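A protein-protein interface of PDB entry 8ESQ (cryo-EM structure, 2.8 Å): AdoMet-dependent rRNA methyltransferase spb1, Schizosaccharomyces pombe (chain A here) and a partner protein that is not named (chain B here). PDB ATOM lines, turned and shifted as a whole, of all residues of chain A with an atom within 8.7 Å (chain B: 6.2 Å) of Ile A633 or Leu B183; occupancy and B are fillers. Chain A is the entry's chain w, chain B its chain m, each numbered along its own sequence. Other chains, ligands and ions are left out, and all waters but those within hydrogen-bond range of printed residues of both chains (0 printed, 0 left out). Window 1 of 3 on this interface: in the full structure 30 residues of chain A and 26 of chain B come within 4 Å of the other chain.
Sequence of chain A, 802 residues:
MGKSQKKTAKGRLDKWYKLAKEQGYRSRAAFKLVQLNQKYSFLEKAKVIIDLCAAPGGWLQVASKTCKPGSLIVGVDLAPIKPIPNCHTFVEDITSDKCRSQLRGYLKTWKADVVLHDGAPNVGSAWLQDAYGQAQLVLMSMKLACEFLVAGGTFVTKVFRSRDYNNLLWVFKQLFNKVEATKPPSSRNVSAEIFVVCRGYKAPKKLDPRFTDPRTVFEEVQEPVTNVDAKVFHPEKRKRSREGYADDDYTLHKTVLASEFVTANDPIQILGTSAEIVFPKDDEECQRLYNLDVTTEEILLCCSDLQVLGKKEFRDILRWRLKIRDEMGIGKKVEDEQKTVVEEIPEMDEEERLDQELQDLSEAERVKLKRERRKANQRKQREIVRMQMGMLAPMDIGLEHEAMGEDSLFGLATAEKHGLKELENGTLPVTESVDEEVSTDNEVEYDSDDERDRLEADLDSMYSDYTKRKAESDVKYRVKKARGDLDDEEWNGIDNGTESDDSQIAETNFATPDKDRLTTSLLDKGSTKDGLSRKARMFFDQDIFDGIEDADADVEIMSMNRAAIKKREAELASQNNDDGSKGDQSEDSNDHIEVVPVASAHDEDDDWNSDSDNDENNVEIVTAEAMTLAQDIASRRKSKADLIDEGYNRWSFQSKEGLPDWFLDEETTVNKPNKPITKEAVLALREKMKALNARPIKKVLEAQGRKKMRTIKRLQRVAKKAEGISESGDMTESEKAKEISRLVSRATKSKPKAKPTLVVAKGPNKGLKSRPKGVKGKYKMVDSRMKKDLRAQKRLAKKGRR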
ATOM      1  N   VAL A 619      11.350 -25.482  20.710  1.00  0.00           N
ATOM      2  CA  VAL A 619      11.015 -26.398  19.628  1.00  0.00           C
ATOM      3  C   VAL A 619      11.675 -25.870  18.365  1.00  0.00           C
ATOM      4  O   VAL A 619      11.819 -24.658  18.183  1.00  0.00           O
ATOM      5  CB  VAL A 619       9.480 -26.554  19.466  1.00  0.00           C
ATOM      6  CG1 VAL A 619       8.857 -25.275  18.947  1.00  0.00           C
ATOM      7  CG2 VAL A 619       9.151 -27.722  18.550  1.00  0.00           C
ATOM      8  N   GLU A 620      12.101 -26.785  17.500  1.00  0.00           N
ATOM      9  CA  GLU A 620      12.789 -26.442  16.256  1.00  0.00           C
ATOM     10  C   GLU A 620      11.998 -27.034  15.097  1.00  0.00           C
ATOM     11  O   GLU A 620      12.063 -28.241  14.844  1.00  0.00           O
ATOM     12  CB  GLU A 620      14.228 -26.953  16.262  1.00  0.00           C
ATOM     13  CG  GLU A 620      15.103 -26.381  17.368  1.00  0.00           C
ATOM     14  CD  GLU A 620      15.066 -27.206  18.639  1.00  0.00           C
ATOM     15  OE1 GLU A 620      13.993 -27.747  18.972  1.00  0.00           O
ATOM     16  OE2 GLU A 620      16.114 -27.317  19.309  1.00  0.00           O
ATOM     17  N   ILE A 621      11.261 -26.188  14.384  1.00  0.00           N
ATOM     18  CA  ILE A 621      10.476 -26.638  13.241  1.00  0.00           C
ATOM     19  C   ILE A 621      11.415 -26.983  12.095  1.00  0.00           C
ATOM     20  O   ILE A 621      11.961 -26.089  11.439  1.00  0.00           O
ATOM     21  CB  ILE A 621       9.459 -25.568  12.812  1.00  0.00           C
ATOM     22  CG1 ILE A 621       8.683 -25.053  14.024  1.00  0.00           C
ATOM     23  CG2 ILE A 621       8.527 -26.121  11.754  1.00  0.00           C
ATOM     24  CD1 ILE A 621       7.816 -23.857  13.720  1.00  0.00           C
ATOM     25  N   VAL A 622      11.609 -28.275  11.842  1.00  0.00           N
ATOM     26  CA  VAL A 622      12.469 -28.724  10.752  1.00  0.00           C
ATOM     27  C   VAL A 622      11.742 -29.604   9.751  1.00  0.00           C
ATOM     28  O   VAL A 622      12.314 -29.912   8.695  1.00  0.00           O
ATOM     29  CB  VAL A 622      13.712 -29.471  11.278  1.00  0.00           C
ATOM     30  CG1 VAL A 622      14.512 -28.591  12.230  1.00  0.00           C
ATOM     31  CG2 VAL A 622      13.308 -30.790  11.904  1.00  0.00           C
ATOM     32  N   THR A 623      10.522 -30.037  10.042  1.00  0.00           N
ATOM     33  CA  THR A 623       9.793 -30.926   9.154  1.00  0.00           C
ATOM     34  C   THR A 623       8.814 -30.132   8.301  1.00  0.00           C
ATOM     35  O   THR A 623       8.309 -29.085   8.712  1.00  0.00           O
ATOM     36  CB  THR A 623       9.036 -31.995   9.943  1.00  0.00           C
ATOM     37  OG1 THR A 623       7.890 -31.407  10.566  1.00  0.00           O
ATOM     38  CG2 THR A 623       9.932 -32.593  11.017  1.00  0.00           C
ATOM     39  N   ALA A 624       8.558 -30.643   7.096  1.00  0.00           N
ATOM     40  CA  ALA A 624       7.537 -30.044   6.247  1.00  0.00           C
ATOM     41  C   ALA A 624       6.167 -30.129   6.905  1.00  0.00           C
ATOM     42  O   ALA A 624       5.359 -29.203   6.792  1.00  0.00           O
ATOM     43  CB  ALA A 624       7.523 -30.726   4.881  1.00  0.00           C
ATOM     44  N   GLU A 625       5.892 -31.236   7.599  1.00  0.00           N
ATOM     45  CA  GLU A 625       4.605 -31.397   8.267  1.00  0.00           C
ATOM     46  C   GLU A 625       4.382 -30.306   9.305  1.00  0.00           C
ATOM     47  O   GLU A 625       3.301 -29.709   9.372  1.00  0.00           O
ATOM     48  CB  GLU A 625       4.526 -32.776   8.921  1.00  0.00           C
ATOM     49  CG  GLU A 625       4.639 -33.944   7.963  1.00  0.00           C
ATOM     50  CD  GLU A 625       4.582 -35.281   8.675  1.00  0.00           C
ATOM     51  OE1 GLU A 625       3.463 -35.751   8.977  1.00  0.00           O
ATOM     52  OE2 GLU A 625       5.655 -35.862   8.940  1.00  0.00           O
ATOM     53  N   ALA A 626       5.395 -30.035  10.130  1.00  0.00           N
ATOM     54  CA  ALA A 626       5.247 -29.026  11.173  1.00  0.00           C
ATOM     55  C   ALA A 626       5.089 -27.633  10.580  1.00  0.00           C
ATOM     56  O   ALA A 626       4.332 -26.809  11.106  1.00  0.00           O
ATOM     57  CB  ALA A 626       6.437 -29.074  12.128  1.00  0.00           C
ATOM     58  N   MET A 627       5.806 -27.346   9.492  1.00  0.00           N
ATOM     59  CA  MET A 627       5.693 -26.034   8.863  1.00  0.00           C
ATOM     60  C   MET A 627       4.296 -25.787   8.311  1.00  0.00           C
ATOM     61  O   MET A 627       3.744 -24.697   8.489  1.00  0.00           O
ATOM     62  CB  MET A 627       6.738 -25.887   7.762  1.00  0.00           C
ATOM     63  CG  MET A 627       7.347 -24.498   7.678  1.00  0.00           C
ATOM     64  SD  MET A 627       7.654 -23.742   9.279  1.00  0.00           S
ATOM     65  CE  MET A 627       8.270 -22.147   8.761  1.00  0.00           C
ATOM     66  N   THR A 628       3.703 -26.782   7.641  1.00  0.00           N
ATOM     67  CA  THR A 628       2.349 -26.602   7.125  1.00  0.00           C
ATOM     68  C   THR A 628       1.376 -26.321   8.258  1.00  0.00           C
ATOM     69  O   THR A 628       0.494 -25.464   8.135  1.00  0.00           O
ATOM     70  CB  THR A 628       1.892 -27.835   6.347  1.00  0.00           C
ATOM     71  OG1 THR A 628       1.770 -28.948   7.241  1.00  0.00           O
ATOM     72  CG2 THR A 628       2.871 -28.177   5.255  1.00  0.00           C
ATOM     73  N   LEU A 629       1.518 -27.044   9.366  1.00  0.00           N
ATOM     74  CA  LEU A 629       0.689 -26.778  10.532  1.00  0.00           C
ATOM     75  C   LEU A 629       0.980 -25.399  11.111  1.00  0.00           C
ATOM     76  O   LEU A 629       0.054 -24.642  11.420  1.00  0.00           O
ATOM     77  CB  LEU A 629       0.914 -27.864  11.576  1.00  0.00           C
ATOM     78  CG  LEU A 629      -0.066 -27.926  12.735  1.00  0.00           C
ATOM     79  CD1 LEU A 629      -1.484 -27.981  12.216  1.00  0.00           C
ATOM     80  CD2 LEU A 629       0.251 -29.156  13.545  1.00  0.00           C
ATOM     81  N   ALA A 630       2.261 -25.051  11.248  1.00  0.00           N
ATOM     82  CA  ALA A 630       2.618 -23.736  11.773  1.00  0.00           C
ATOM     83  C   ALA A 630       2.156 -22.625  10.841  1.00  0.00           C
ATOM     84  O   ALA A 630       1.699 -21.572  11.302  1.00  0.00           O
ATOM     85  CB  ALA A 630       4.125 -23.651  12.002  1.00  0.00           C
ATOM     86  N   GLN A 631       2.274 -22.835   9.529  1.00  0.00           N
ATOM     87  CA  GLN A 631       1.787 -21.841   8.579  1.00  0.00           C
ATOM     88  C   GLN A 631       0.280 -21.660   8.697  1.00  0.00           C
ATOM     89  O   GLN A 631      -0.222 -20.534   8.629  1.00  0.00           O
ATOM     90  CB  GLN A 631       2.175 -22.237   7.156  1.00  0.00           C
ATOM     91  CG  GLN A 631       3.624 -21.947   6.815  1.00  0.00           C
ATOM     92  CD  GLN A 631       3.932 -22.159   5.348  1.00  0.00           C
ATOM     93  OE1 GLN A 631       3.088 -22.629   4.588  1.00  0.00           O
ATOM     94  NE2 GLN A 631       5.145 -21.807   4.942  1.00  0.00           N
ATOM     95  N   ASP A 632      -0.455 -22.757   8.879  1.00  0.00           N
ATOM     96  CA  ASP A 632      -1.904 -22.664   9.027  1.00  0.00           C
ATOM     97  C   ASP A 632      -2.281 -21.913  10.298  1.00  0.00           C
ATOM     98  O   ASP A 632      -3.253 -21.149  10.314  1.00  0.00           O
ATOM     99  CB  ASP A 632      -2.521 -24.062   9.016  1.00  0.00           C
ATOM    100  CG  ASP A 632      -2.612 -24.646   7.617  1.00  0.00           C
ATOM    101  OD1 ASP A 632      -2.467 -23.879   6.642  1.00  0.00           O
ATOM    102  OD2 ASP A 632      -2.830 -25.871   7.491  1.00  0.00           O
ATOM    103  N   ILE A 633      -1.530 -22.127  11.381  1.00  0.00           N
ATOM    104  CA  ILE A 633      -1.803 -21.409  12.625  1.00  0.00           C
ATOM    105  C   ILE A 633      -1.557 -19.916  12.445  1.00  0.00           C
ATOM    106  O   ILE A 633      -2.392 -19.082  12.812  1.00  0.00           O
ATOM    107  CB  ILE A 633      -0.959 -21.978  13.778  1.00  0.00           C
ATOM    108  CG1 ILE A 633      -1.217 -23.474  13.954  1.00  0.00           C
ATOM    109  CG2 ILE A 633      -1.253 -21.234  15.067  1.00  0.00           C
ATOM    110  CD1 ILE A 633      -0.323 -24.128  14.982  1.00  0.00           C
ATOM    111  N   ALA A 634      -0.403 -19.556  11.879  1.00  0.00           N
ATOM    112  CA  ALA A 634      -0.046 -18.146  11.762  1.00  0.00           C
ATOM    113  C   ALA A 634      -0.883 -17.446  10.700  1.00  0.00           C
ATOM    114  O   ALA A 634      -1.378 -16.335  10.920  1.00  0.00           O
ATOM    115  CB  ALA A 634       1.442 -18.005  11.450  1.00  0.00           C
ATOM    116  N   SER A 635      -1.056 -18.082   9.541  1.00  0.00           N
ATOM    117  CA  SER A 635      -1.805 -17.454   8.460  1.00  0.00           C
ATOM    118  C   SER A 635      -3.301 -17.399   8.732  1.00  0.00           C
ATOM    119  O   SER A 635      -4.042 -16.888   7.887  1.00  0.00           O
ATOM    120  CB  SER A 635      -1.555 -18.180   7.140  1.00  0.00           C
ATOM    121  OG  SER A 635      -2.398 -19.310   7.013  1.00  0.00           O
ATOM    122  N   ARG A 636      -3.767 -17.946   9.854  1.00  0.00           N
ATOM    123  CA  ARG A 636      -5.163 -17.924  10.278  1.00  0.00           C
ATOM    124  C   ARG A 636      -6.087 -18.611   9.284  1.00  0.00           C
ATOM    125  O   ARG A 636      -7.304 -18.588   9.482  1.00  0.00           O
ATOM    126  CB  ARG A 636      -5.680 -16.501  10.530  1.00  0.00           C
ATOM    127  CG  ARG A 636      -4.869 -15.707  11.537  1.00  0.00           C
ATOM    128  CD  ARG A 636      -5.038 -16.266  12.938  1.00  0.00           C
ATOM    129  NE  ARG A 636      -4.369 -15.446  13.941  1.00  0.00           N
ATOM    130  CZ  ARG A 636      -4.242 -15.780  15.217  1.00  0.00           C
ATOM    131  NH1 ARG A 636      -4.732 -16.916  15.686  1.00  0.00           N
ATOM    132  NH2 ARG A 636      -3.608 -14.953  16.044  1.00  0.00           N
ATOM    133  N   ARG A 637      -5.553 -19.222   8.223  1.00  0.00           N
ATOM    134  CA  ARG A 637      -6.401 -19.862   7.224  1.00  0.00           C
ATOM    135  C   ARG A 637      -7.265 -20.944   7.854  1.00  0.00           C
ATOM    136  O   ARG A 637      -8.466 -21.033   7.576  1.00  0.00           O
ATOM    137  CB  ARG A 637      -5.533 -20.440   6.106  1.00  0.00           C
ATOM    138  CG  ARG A 637      -6.282 -20.764   4.827  1.00  0.00           C
ATOM    139  CD  ARG A 637      -6.667 -22.231   4.773  1.00  0.00           C
ATOM    140  NE  ARG A 637      -5.496 -23.098   4.792  1.00  0.00           N
ATOM    141  CZ  ARG A 637      -5.537 -24.405   5.010  1.00  0.00           C
ATOM    142  NH1 ARG A 637      -6.679 -25.034   5.233  1.00  0.00           N
ATOM    143  NH2 ARG A 637      -4.401 -25.099   5.007  1.00  0.00           N
ATOM    144  N   LYS A 638      -6.675 -21.765   8.714  1.00  0.00           N
ATOM    145  CA  LYS A 638      -7.398 -22.785   9.456  1.00  0.00           C
ATOM    146  C   LYS A 638      -7.554 -22.303  10.893  1.00  0.00           C
ATOM    147  O   LYS A 638      -6.560 -21.972  11.549  1.00  0.00           O
ATOM    148  CB  LYS A 638      -6.653 -24.118   9.398  1.00  0.00           C
ATOM    149  CG  LYS A 638      -7.297 -25.246  10.178  1.00  0.00           C
ATOM    150  CD  LYS A 638      -8.717 -25.514   9.722  1.00  0.00           C
ATOM    151  CE  LYS A 638      -9.087 -26.970   9.950  1.00  0.00           C
ATOM    152  NZ  LYS A 638      -9.052 -27.341  11.389  1.00  0.00           N
ATOM    153  N   SER A 639      -8.796 -22.250  11.367  1.00  0.00           N
ATOM    154  CA  SER A 639      -9.071 -21.714  12.694  1.00  0.00           C
ATOM    155  C   SER A 639      -8.345 -22.519  13.763  1.00  0.00           C
ATOM    156  O   SER A 639      -8.245 -23.746  13.680  1.00  0.00           O
ATOM    157  CB  SER A 639     -10.574 -21.717  12.962  1.00  0.00           C
ATOM    158  OG  SER A 639     -10.849 -21.437  14.323  1.00  0.00           O
ATOM    159  N   LYS A 640      -7.826 -21.816  14.770  1.00  0.00           N
ATOM    160  CA  LYS A 640      -7.098 -22.487  15.842  1.00  0.00           C
ATOM    161  C   LYS A 640      -8.001 -23.442  16.611  1.00  0.00           C
ATOM    162  O   LYS A 640      -7.584 -24.548  16.972  1.00  0.00           O
ATOM    163  CB  LYS A 640      -6.484 -21.457  16.787  1.00  0.00           C
ATOM    164  CG  LYS A 640      -5.663 -22.067  17.907  1.00  0.00           C
ATOM    165  CD  LYS A 640      -5.171 -21.006  18.870  1.00  0.00           C
ATOM    166  CE  LYS A 640      -4.066 -20.168  18.256  1.00  0.00           C
ATOM    167  NZ  LYS A 640      -3.481 -19.229  19.251  1.00  0.00           N
ATOM    168  N   ALA A 641      -9.243 -23.030  16.874  1.00  0.00           N
ATOM    169  CA  ALA A 641     -10.176 -23.900  17.580  1.00  0.00           C
ATOM    170  C   ALA A 641     -10.468 -25.160  16.776  1.00  0.00           C
ATOM    171  O   ALA A 641     -10.597 -26.251  17.343  1.00  0.00           O
ATOM    172  CB  ALA A 641     -11.469 -23.146  17.887  1.00  0.00           C
ATOM    173  N   LEU A 643      -8.384 -26.523  14.666  1.00  0.00           N
ATOM    174  CA  LEU A 643      -7.173 -27.336  14.732  1.00  0.00           C
ATOM    175  C   LEU A 643      -7.129 -28.162  16.010  1.00  0.00           C
ATOM    176  O   LEU A 643      -6.717 -29.326  15.990  1.00  0.00           O
ATOM    177  CB  LEU A 643      -5.933 -26.451  14.637  1.00  0.00           C
ATOM    178  CG  LEU A 643      -5.626 -25.823  13.281  1.00  0.00           C
ATOM    179  CD1 LEU A 643      -4.775 -24.583  13.461  1.00  0.00           C
ATOM    180  CD2 LEU A 643      -4.936 -26.827  12.383  1.00  0.00           C
ATOM    181  N   ILE A 644      -7.534 -27.570  17.134  1.00  0.00           N
ATOM    182  CA  ILE A 644      -7.536 -28.299  18.399  1.00  0.00           C
ATOM    183  C   ILE A 644      -8.503 -29.473  18.334  1.00  0.00           C
ATOM    184  O   ILE A 644      -8.181 -30.590  18.753  1.00  0.00           O
ATOM    185  CB  ILE A 644      -7.872 -27.352  19.564  1.00  0.00           C
ATOM    186  CG1 ILE A 644      -6.774 -26.300  19.726  1.00  0.00           C
ATOM    187  CG2 ILE A 644      -8.049 -28.131  20.853  1.00  0.00           C
ATOM    188  CD1 ILE A 644      -7.140 -25.179  20.671  1.00  0.00           C
ATOM    189  N   LYS A 688      14.986 -21.645   5.809  1.00  0.00           N
ATOM    190  CA  LYS A 688      15.619 -21.888   7.103  1.00  0.00           C
ATOM    191  C   LYS A 688      16.947 -22.614   6.944  1.00  0.00           C
ATOM    192  O   LYS A 688      17.943 -22.253   7.582  1.00  0.00           O
ATOM    193  CB  LYS A 688      14.688 -22.691   8.008  1.00  0.00           C
ATOM    194  CG  LYS A 688      13.450 -21.958   8.484  1.00  0.00           C
ATOM    195  CD  LYS A 688      12.991 -22.524   9.820  1.00  0.00           C
ATOM    196  CE  LYS A 688      12.252 -21.493  10.652  1.00  0.00           C
ATOM    197  NZ  LYS A 688      11.882 -22.022  11.993  1.00  0.00           N
ATOM    198  N   LEU B 175       4.964 -17.236  15.484  1.00  0.00           N
ATOM    199  CA  LEU B 175       4.211 -17.971  16.489  1.00  0.00           C
ATOM    200  C   LEU B 175       4.629 -17.552  17.891  1.00  0.00           C
ATOM    201  O   LEU B 175       5.818 -17.411  18.187  1.00  0.00           O
ATOM    202  CB  LEU B 175       4.418 -19.473  16.312  1.00  0.00           C
ATOM    203  CG  LEU B 175       4.039 -20.069  14.957  1.00  0.00           C
ATOM    204  CD1 LEU B 175       3.964 -21.579  15.052  1.00  0.00           C
ATOM    205  CD2 LEU B 175       2.715 -19.504  14.485  1.00  0.00           C
ATOM    206  N   GLU B 178       2.510 -19.851  23.280  1.00  0.00           N
ATOM    207  CA  GLU B 178       1.373 -20.763  23.349  1.00  0.00           C
ATOM    208  C   GLU B 178       1.086 -21.397  21.993  1.00  0.00           C
ATOM    209  O   GLU B 178       0.736 -22.581  21.917  1.00  0.00           O
ATOM    210  CB  GLU B 178       0.142 -20.032  23.887  1.00  0.00           C
ATOM    211  CG  GLU B 178      -0.291 -18.822  23.079  1.00  0.00           C
ATOM    212  CD  GLU B 178      -1.366 -19.155  22.064  1.00  0.00           C
ATOM    213  OE1 GLU B 178      -1.952 -20.253  22.156  1.00  0.00           O
ATOM    214  OE2 GLU B 178      -1.628 -18.316  21.177  1.00  0.00           O
ATOM    215  N   GLU B 179       1.225 -20.628  20.910  1.00  0.00           N
ATOM    216  CA  GLU B 179       1.058 -21.202  19.578  1.00  0.00           C
ATOM    217  C   GLU B 179       2.152 -22.217  19.282  1.00  0.00           C
ATOM    218  O   GLU B 179       1.910 -23.222  18.604  1.00  0.00           O
ATOM    219  CB  GLU B 179       1.051 -20.097  18.524  1.00  0.00           C
ATOM    220  CG  GLU B 179      -0.298 -19.432  18.339  1.00  0.00           C
ATOM    221  CD  GLU B 179      -0.180 -17.989  17.893  1.00  0.00           C
ATOM    222  OE1 GLU B 179       0.935 -17.571  17.516  1.00  0.00           O
ATOM    223  OE2 GLU B 179      -1.203 -17.274  17.916  1.00  0.00           O
ATOM    224  N   LEU B 180       3.367 -21.963  19.769  1.00  0.00           N
ATOM    225  CA  LEU B 180       4.444 -22.933  19.608  1.00  0.00           C
ATOM    226  C   LEU B 180       4.148 -24.212  20.380  1.00  0.00           C
ATOM    227  O   LEU B 180       4.454 -25.313  19.912  1.00  0.00           O
ATOM    228  CB  LEU B 180       5.767 -22.320  20.061  1.00  0.00           C
ATOM    229  CG  LEU B 180       6.689 -21.792  18.961  1.00  0.00           C
ATOM    230  CD1 LEU B 180       8.126 -21.805  19.436  1.00  0.00           C
ATOM    231  CD2 LEU B 180       6.540 -22.607  17.685  1.00  0.00           C
ATOM    232  N   GLY B 181       3.561 -24.083  21.571  1.00  0.00           N
ATOM    233  CA  GLY B 181       3.168 -25.266  22.319  1.00  0.00           C
ATOM    234  C   GLY B 181       2.078 -26.059  21.626  1.00  0.00           C
ATOM    235  O   GLY B 181       2.141 -27.288  21.555  1.00  0.00           O
ATOM    236  N   LEU B 182       1.062 -25.366  21.106  1.00  0.00           N
ATOM    237  CA  LEU B 182      -0.003 -26.048  20.376  1.00  0.00           C
ATOM    238  C   LEU B 182       0.544 -26.778  19.160  1.00  0.00           C
ATOM    239  O   LEU B 182       0.159 -27.919  18.887  1.00  0.00           O
ATOM    240  CB  LEU B 182      -1.079 -25.050  19.953  1.00  0.00           C
ATOM    241  CG  LEU B 182      -2.301 -24.939  20.862  1.00  0.00           C
ATOM    242  CD1 LEU B 182      -3.087 -26.236  20.828  1.00  0.00           C
ATOM    243  CD2 LEU B 182      -1.892 -24.593  22.280  1.00  0.00           C
ATOM    244  N   LEU B 183       1.437 -26.131  18.411  1.00  0.00           N
ATOM    245  CA  LEU B 183       2.069 -26.798  17.281  1.00  0.00           C
ATOM    246  C   LEU B 183       2.879 -28.001  17.743  1.00  0.00           C
ATOM    247  O   LEU B 183       2.905 -29.036  17.069  1.00  0.00           O
ATOM    248  CB  LEU B 183       2.956 -25.816  16.520  1.00  0.00           C
ATOM    249  CG  LEU B 183       3.887 -26.440  15.482  1.00  0.00           C
ATOM    250  CD1 LEU B 183       3.171 -26.619  14.160  1.00  0.00           C
ATOM    251  CD2 LEU B 183       5.129 -25.594  15.313  1.00  0.00           C
ATOM    252  N   LYS B 184       3.544 -27.882  18.892  1.00  0.00           N
ATOM    253  CA  LYS B 184       4.323 -28.998  19.418  1.00  0.00           C
ATOM    254  C   LYS B 184       3.439 -30.214  19.665  1.00  0.00           C
ATOM    255  O   LYS B 184       3.759 -31.328  19.235  1.00  0.00           O
ATOM    256  CB  LYS B 184       5.033 -28.574  20.704  1.00  0.00           C
ATOM    257  CG  LYS B 184       6.173 -29.485  21.123  1.00  0.00           C
ATOM    258  CD  LYS B 184       5.697 -30.559  22.080  1.00  0.00           C
ATOM    259  CE  LYS B 184       5.341 -29.975  23.433  1.00  0.00           C
ATOM    260  NZ  LYS B 184       4.833 -31.017  24.367  1.00  0.00           N
ATOM    261  N   ARG B 185       2.315 -30.017  20.355  1.00  0.00           N
ATOM    262  CA  ARG B 185       1.422 -31.133  20.646  1.00  0.00           C
ATOM    263  C   ARG B 185       0.773 -31.667  19.376  1.00  0.00           C
ATOM    264  O   ARG B 185       0.733 -32.882  19.151  1.00  0.00           O
ATOM    265  CB  ARG B 185       0.363 -30.704  21.657  1.00  0.00           C
ATOM    266  CG  ARG B 185       0.931 -30.067  22.909  1.00  0.00           C
ATOM    267  CD  ARG B 185      -0.110 -29.989  24.001  1.00  0.00           C
ATOM    268  NE  ARG B 185      -0.507 -31.312  24.465  1.00  0.00           N
ATOM    269  CZ  ARG B 185      -0.059 -31.885  25.573  1.00  0.00           C
ATOM    270  NH1 ARG B 185       0.802 -31.271  26.368  1.00  0.00           N
ATOM    271  NH2 ARG B 185      -0.486 -33.102  25.892  1.00  0.00           N
ATOM    272  N   LEU B 186       0.260 -30.773  18.529  1.00  0.00           N
ATOM    273  CA  LEU B 186      -0.423 -31.211  17.316  1.00  0.00           C
ATOM    274  C   LEU B 186       0.521 -31.940  16.367  1.00  0.00           C
ATOM    275  O   LEU B 186       0.155 -32.971  15.792  1.00  0.00           O
ATOM    276  CB  LEU B 186      -1.066 -30.018  16.616  1.00  0.00           C
ATOM    277  CG  LEU B 186      -2.296 -29.383  17.259  1.00  0.00           C
ATOM    278  CD1 LEU B 186      -2.840 -28.278  16.372  1.00  0.00           C
ATOM    279  CD2 LEU B 186      -3.355 -30.437  17.508  1.00  0.00           C
ATOM    280  N   ALA B 187       1.736 -31.421  16.182  1.00  0.00           N
ATOM    281  CA  ALA B 187       2.664 -32.038  15.241  1.00  0.00           C
ATOM    282  C   ALA B 187       3.277 -33.324  15.773  1.00  0.00           C
ATOM    283  O   ALA B 187       3.781 -34.126  14.980  1.00  0.00           O
ATOM    284  CB  ALA B 187       3.779 -31.059  14.869  1.00  0.00           C
ATOM    285  N   GLN B 188       3.257 -33.536  17.085  1.00  0.00           N
ATOM    286  CA  GLN B 188       3.723 -34.783  17.671  1.00  0.00           C
ATOM    287  C   GLN B 188       2.593 -35.771  17.911  1.00  0.00           C
ATOM    288  O   GLN B 188       2.839 -36.845  18.469  1.00  0.00           O
ATOM    289  CB  GLN B 188       4.461 -34.511  18.983  1.00  0.00           C
ATOM    290  CG  GLN B 188       5.829 -33.884  18.802  1.00  0.00           C
ATOM    291  CD  GLN B 188       6.699 -34.030  20.032  1.00  0.00           C
ATOM    292  OE1 GLN B 188       6.270 -33.743  21.148  1.00  0.00           O
ATOM    293  NE2 GLN B 188       7.930 -34.483  19.834  1.00  0.00           N
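Of the printed residues of chain B, Val A619 touches Leu B180 (3.6 Å). Of the printed residues of chain B, Ile A621 touches Leu B183. Thr A623 touches none of the printed residues of chain B. Of the printed residues of chain B, Ile A633 touches Glu B179 and Leu B183. Of the printed residues of chain B, Lys A640 touches Glu B178 and Glu B179. Of the printed residues of chain A, Leu B175 touches Ala A630 and Ala A634. Printed residues of chain A within 4 Å of Leu B180: Val A619. No residue of chain A comes within 4 Å of Gly B181. The nearest printed residue of chain A that does not touch Leu B183 is Val A619 (5.2 Å). The nearest printed residue of chain B that does not touch Ile A644 is Leu B186 (4.8 Å).
Hydrophobic or aromatic side chains of chain B that line the printed part of chain A: Leu B175, Leu B180, Leu B182, Leu B183 and Leu B186. Along chain B the printed residues that touch a printed residue of chain A span positions 175 to 187.
N of Ala A626 is in hydrogen-bond range of OG1 of Thr A623 (2.9 Å).
The side-chain carboxylate (OE2) of Glu B179 is in salt-bridge range of the side-chain amino group (NZ) of Lys A640, at 3.3 Å. The guanidinium group (NH2) of Arg A636 is in salt-bridge range of the side-chain carboxylate (OE2) of Glu B179. The side-chain carboxylate (OE2) of Glu B178 lies within salt-bridge range of the side-chain amino group (NZ) of Lys A640 (2.8 Å).
Val A619 touches Leu B180. Ile A621 touches Leu B183 (CD1 to CD2, 3.6 Å). Leu A629 touches Leu B183. Leu A629 touches Leu B186. Ala B187 touches Leu A629 (N to CD2, 3.8 Å). CB of Ala A630 touches CD1 of Leu B175 (3.7 Å). N of Ala A630 touches CD1 of Leu B183, at 3.4 Å. Glu B179 touches Ile A633. Ala A634 touches Leu B175 (CB to CD2, 3.6 Å). CG1 of Ile A644 touches CD1 of Leu B182, at 3.8 Å.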
